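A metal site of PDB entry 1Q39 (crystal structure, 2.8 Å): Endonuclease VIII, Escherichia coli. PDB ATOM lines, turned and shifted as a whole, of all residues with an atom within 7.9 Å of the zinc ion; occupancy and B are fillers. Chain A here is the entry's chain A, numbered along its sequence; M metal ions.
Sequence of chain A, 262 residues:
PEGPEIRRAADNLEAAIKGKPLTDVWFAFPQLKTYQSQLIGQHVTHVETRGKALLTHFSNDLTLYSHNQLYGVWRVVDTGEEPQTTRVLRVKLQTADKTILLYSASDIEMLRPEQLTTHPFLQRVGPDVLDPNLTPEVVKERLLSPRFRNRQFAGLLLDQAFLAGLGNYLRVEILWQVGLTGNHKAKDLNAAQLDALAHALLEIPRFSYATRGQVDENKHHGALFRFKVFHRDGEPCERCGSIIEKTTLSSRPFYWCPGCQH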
ATOM      1  N   TRP A 176     -12.151   6.576 -31.834  1.00  0.00           N
ATOM      2  CA  TRP A 176     -12.689   7.045 -30.564  1.00  0.00           C
ATOM      3  C   TRP A 176     -13.110   8.509 -30.651  1.00  0.00           C
ATOM      4  O   TRP A 176     -13.963   8.945 -29.881  1.00  0.00           O
ATOM      5  CB  TRP A 176     -11.654   6.902 -29.443  1.00  0.00           C
ATOM      6  CG  TRP A 176     -12.149   7.459 -28.136  1.00  0.00           C
ATOM      7  CD1 TRP A 176     -12.947   6.841 -27.223  1.00  0.00           C
ATOM      8  CD2 TRP A 176     -11.893   8.779 -27.614  1.00  0.00           C
ATOM      9  NE1 TRP A 176     -13.210   7.672 -26.168  1.00  0.00           N
ATOM     10  CE2 TRP A 176     -12.577   8.875 -26.373  1.00  0.00           C
ATOM     11  CE3 TRP A 176     -11.147   9.881 -28.064  1.00  0.00           C
ATOM     12  CZ2 TRP A 176     -12.540  10.033 -25.577  1.00  0.00           C
ATOM     13  CZ3 TRP A 176     -11.128  11.033 -27.282  1.00  0.00           C
ATOM     14  CH2 TRP A 176     -11.819  11.095 -26.047  1.00  0.00           C
ATOM     15  N   VAL A 229      -7.400   5.947 -25.815  1.00  0.00           N
ATOM     16  CA  VAL A 229      -7.742   4.542 -25.652  1.00  0.00           C
ATOM     17  C   VAL A 229      -6.615   3.563 -25.966  1.00  0.00           C
ATOM     18  O   VAL A 229      -6.694   2.375 -25.647  1.00  0.00           O
ATOM     19  CB  VAL A 229      -8.961   4.167 -26.520  1.00  0.00           C
ATOM     20  CG1 VAL A 229     -10.160   5.040 -26.122  1.00  0.00           C
ATOM     21  CG2 VAL A 229      -8.603   4.294 -27.997  1.00  0.00           C
ATOM     22  N   PRO A 236     -10.578   4.878 -17.059  1.00  0.00           N
ATOM     23  CA  PRO A 236     -11.847   5.458 -17.517  1.00  0.00           C
ATOM     24  C   PRO A 236     -11.696   6.263 -18.806  1.00  0.00           C
ATOM     25  O   PRO A 236     -10.598   6.665 -19.178  1.00  0.00           O
ATOM     26  CB  PRO A 236     -12.280   6.336 -16.343  1.00  0.00           C
ATOM     27  CG  PRO A 236     -11.468   5.807 -15.160  1.00  0.00           C
ATOM     28  CD  PRO A 236     -10.154   5.484 -15.791  1.00  0.00           C
ATOM     29  N   CYS A 237     -12.816   6.481 -19.476  1.00  0.00           N
ATOM     30  CA  CYS A 237     -12.858   7.247 -20.705  1.00  0.00           C
ATOM     31  C   CYS A 237     -13.164   8.728 -20.421  1.00  0.00           C
ATOM     32  O   CYS A 237     -14.246   9.074 -19.975  1.00  0.00           O
ATOM     33  CB  CYS A 237     -13.908   6.643 -21.638  1.00  0.00           C
ATOM     34  SG  CYS A 237     -14.474   7.743 -22.931  1.00  0.00           S
ATOM     35  N   GLU A 238     -12.179   9.585 -20.668  1.00  0.00           N
ATOM     36  CA  GLU A 238     -12.312  11.024 -20.473  1.00  0.00           C
ATOM     37  C   GLU A 238     -13.681  11.571 -20.871  1.00  0.00           C
ATOM     38  O   GLU A 238     -14.069  12.645 -20.419  1.00  0.00           O
ATOM     39  CB  GLU A 238     -11.231  11.732 -21.293  1.00  0.00           C
ATOM     40  CG  GLU A 238     -11.461  13.218 -21.494  1.00  0.00           C
ATOM     41  CD  GLU A 238     -10.681  13.758 -22.671  1.00  0.00           C
ATOM     42  OE1 GLU A 238     -10.878  13.244 -23.801  1.00  0.00           O
ATOM     43  OE2 GLU A 238      -9.873  14.690 -22.478  1.00  0.00           O
ATOM     44  N   ARG A 239     -14.393  10.828 -21.716  1.00  0.00           N
ATOM     45  CA  ARG A 239     -15.699  11.242 -22.217  1.00  0.00           C
ATOM     46  C   ARG A 239     -16.865  10.840 -21.313  1.00  0.00           C
ATOM     47  O   ARG A 239     -17.477  11.684 -20.657  1.00  0.00           O
ATOM     48  CB  ARG A 239     -15.898  10.635 -23.609  1.00  0.00           C
ATOM     49  CG  ARG A 239     -16.375  11.598 -24.683  1.00  0.00           C
ATOM     50  CD  ARG A 239     -17.781  12.080 -24.419  1.00  0.00           C
ATOM     51  NE  ARG A 239     -18.520  12.337 -25.657  1.00  0.00           N
ATOM     52  CZ  ARG A 239     -18.862  11.379 -26.515  1.00  0.00           C
ATOM     53  NH1 ARG A 239     -18.522  10.118 -26.274  1.00  0.00           N
ATOM     54  NH2 ARG A 239     -19.545  11.676 -27.628  1.00  0.00           N
ATOM     55  N   CYS A 240     -17.156   9.537 -21.264  1.00  0.00           N
ATOM     56  CA  CYS A 240     -18.240   9.014 -20.461  1.00  0.00           C
ATOM     57  C   CYS A 240     -17.845   8.328 -19.145  1.00  0.00           C
ATOM     58  O   CYS A 240     -18.673   8.181 -18.246  1.00  0.00           O
ATOM     59  CB  CYS A 240     -19.077   8.045 -21.306  1.00  0.00           C
ATOM     60  SG  CYS A 240     -18.256   6.497 -21.770  1.00  0.00           S
ATOM     61  N   GLY A 241     -16.594   7.895 -19.043  1.00  0.00           N
ATOM     62  CA  GLY A 241     -16.142   7.252 -17.810  1.00  0.00           C
ATOM     63  C   GLY A 241     -16.136   5.734 -17.810  1.00  0.00           C
ATOM     64  O   GLY A 241     -15.756   5.107 -16.820  1.00  0.00           O
ATOM     65  N   SER A 242     -16.555   5.127 -18.918  1.00  0.00           N
ATOM     66  CA  SER A 242     -16.606   3.673 -19.018  1.00  0.00           C
ATOM     67  C   SER A 242     -15.191   3.108 -19.040  1.00  0.00           C
ATOM     68  O   SER A 242     -14.260   3.780 -19.488  1.00  0.00           O
ATOM     69  CB  SER A 242     -17.335   3.258 -20.297  1.00  0.00           C
ATOM     70  OG  SER A 242     -18.568   3.932 -20.411  1.00  0.00           O
ATOM     71  N   ILE A 243     -15.031   1.882 -18.546  1.00  0.00           N
ATOM     72  CA  ILE A 243     -13.715   1.272 -18.533  1.00  0.00           C
ATOM     73  C   ILE A 243     -13.391   0.809 -19.944  1.00  0.00           C
ATOM     74  O   ILE A 243     -14.120  -0.017 -20.515  1.00  0.00           O
ATOM     75  CB  ILE A 243     -13.633   0.064 -17.582  1.00  0.00           C
ATOM     76  CG1 ILE A 243     -13.868   0.511 -16.135  1.00  0.00           C
ATOM     77  CG2 ILE A 243     -12.251  -0.587 -17.696  1.00  0.00           C
ATOM     78  CD1 ILE A 243     -12.756   1.355 -15.555  1.00  0.00           C
ATOM     79  N   ILE A 244     -12.315   1.363 -20.492  1.00  0.00           N
ATOM     80  CA  ILE A 244     -11.845   1.072 -21.834  1.00  0.00           C
ATOM     81  C   ILE A 244     -11.414  -0.384 -21.933  1.00  0.00           C
ATOM     82  O   ILE A 244     -10.644  -0.864 -21.113  1.00  0.00           O
ATOM     83  CB  ILE A 244     -10.677   2.035 -22.175  1.00  0.00           C
ATOM     84  CG1 ILE A 244     -11.200   3.473 -22.166  1.00  0.00           C
ATOM     85  CG2 ILE A 244     -10.069   1.701 -23.544  1.00  0.00           C
ATOM     86  CD1 ILE A 244     -10.119   4.544 -22.137  1.00  0.00           C
ATOM     87  N   TRP A 256     -10.979   0.495 -27.403  1.00  0.00           N
ATOM     88  CA  TRP A 256     -12.152   1.336 -27.546  1.00  0.00           C
ATOM     89  C   TRP A 256     -12.891   1.496 -26.220  1.00  0.00           C
ATOM     90  O   TRP A 256     -12.566   0.838 -25.224  1.00  0.00           O
ATOM     91  CB  TRP A 256     -13.088   0.731 -28.592  1.00  0.00           C
ATOM     92  CG  TRP A 256     -14.011  -0.307 -28.056  1.00  0.00           C
ATOM     93  CD1 TRP A 256     -15.315  -0.136 -27.665  1.00  0.00           C
ATOM     94  CD2 TRP A 256     -13.700  -1.686 -27.827  1.00  0.00           C
ATOM     95  NE1 TRP A 256     -15.836  -1.317 -27.195  1.00  0.00           N
ATOM     96  CE2 TRP A 256     -14.867  -2.290 -27.289  1.00  0.00           C
ATOM     97  CE3 TRP A 256     -12.565  -2.473 -28.017  1.00  0.00           C
ATOM     98  CZ2 TRP A 256     -14.918  -3.644 -26.947  1.00  0.00           C
ATOM     99  CZ3 TRP A 256     -12.617  -3.828 -27.675  1.00  0.00           C
ATOM    100  CH2 TRP A 256     -13.786  -4.396 -27.140  1.00  0.00           C
ATOM    101  N   CYS A 257     -13.860   2.394 -26.191  1.00  0.00           N
ATOM    102  CA  CYS A 257     -14.647   2.606 -24.999  1.00  0.00           C
ATOM    103  C   CYS A 257     -16.034   2.028 -25.275  1.00  0.00           C
ATOM    104  O   CYS A 257     -16.826   2.612 -26.023  1.00  0.00           O
ATOM    105  CB  CYS A 257     -14.757   4.095 -24.693  1.00  0.00           C
ATOM    106  SG  CYS A 257     -16.056   4.461 -23.502  1.00  0.00           S
ATOM    107  N   PRO A 258     -16.349   0.863 -24.684  1.00  0.00           N
ATOM    108  CA  PRO A 258     -17.663   0.234 -24.899  1.00  0.00           C
ATOM    109  C   PRO A 258     -18.796   1.159 -24.485  1.00  0.00           C
ATOM    110  O   PRO A 258     -19.964   0.924 -24.801  1.00  0.00           O
ATOM    111  CB  PRO A 258     -17.600  -1.025 -24.041  1.00  0.00           C
ATOM    112  CG  PRO A 258     -16.684  -0.614 -22.919  1.00  0.00           C
ATOM    113  CD  PRO A 258     -15.597   0.139 -23.642  1.00  0.00           C
ATOM    114  N   GLY A 259     -18.413   2.243 -23.801  1.00  0.00           N
ATOM    115  CA  GLY A 259     -19.378   3.212 -23.338  1.00  0.00           C
ATOM    116  C   GLY A 259     -19.904   4.184 -24.387  1.00  0.00           C
ATOM    117  O   GLY A 259     -21.110   4.238 -24.633  1.00  0.00           O
ATOM    118  N   CYS A 260     -19.015   4.952 -25.015  1.00  0.00           N
ATOM    119  CA  CYS A 260     -19.470   5.924 -26.005  1.00  0.00           C
ATOM    120  C   CYS A 260     -19.141   5.627 -27.478  1.00  0.00           C
ATOM    121  O   CYS A 260     -19.359   6.478 -28.346  1.00  0.00           O
ATOM    122  CB  CYS A 260     -18.961   7.312 -25.610  1.00  0.00           C
ATOM    123  SG  CYS A 260     -17.215   7.381 -25.251  1.00  0.00           S
ATOM    124  N   GLN A 261     -18.637   4.430 -27.741  1.00  0.00           N
ATOM    125  CA  GLN A 261     -18.327   3.995 -29.111  1.00  0.00           C
ATOM    126  C   GLN A 261     -19.281   2.853 -29.465  1.00  0.00           C
ATOM    127  O   GLN A 261     -19.388   1.873 -28.713  1.00  0.00           O
ATOM    128  CB  GLN A 261     -16.869   3.530 -29.215  1.00  0.00           C
ATOM    129  CG  GLN A 261     -15.877   4.629 -29.627  1.00  0.00           C
ATOM    130  CD  GLN A 261     -14.414   4.171 -29.582  1.00  0.00           C
ATOM    131  OE1 GLN A 261     -13.738   4.275 -28.543  1.00  0.00           O
ATOM    132  NE2 GLN A 261     -13.925   3.655 -30.711  1.00  0.00           N
HETATM  133 ZN    ZN M   1     -16.451   6.722 -23.388  1.00  0.00          ZN
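SG of Cys 240 sits close to OG of Ser 242. N of Cys 257 sits at hydrogen-bond distance from OE1 of Gln 261 (3.0 Å). O of Ser 242 lies within hydrogen-bond range of N of Cys 237. SG of Cys 260 lies close to NH1 of Arg 239 (3.2 Å). SG of Cys 257 lies close to N of Gly 259, at 3.3 Å. The side-chain sulfur (SG) of Cys 237 lies close to the backbone NH (N) of Arg 239 (3.3 Å). NE1 of Trp 176 lies close to SG of Cys 237 (3.5 Å).
Merely in contact with the zinc ion: Arg 239. Of the 17 residues printed, 5 come within 4 Å of the zinc ion. The nearest printed residue that does not touch the zinc ion is Trp 176 (4.4 Å).
The zinc ion is bound by SG of Cys 260, SG of Cys 237, SG of Cys 257 and SG of Cys 240. The zinc ion has four donor atoms within binding distance.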
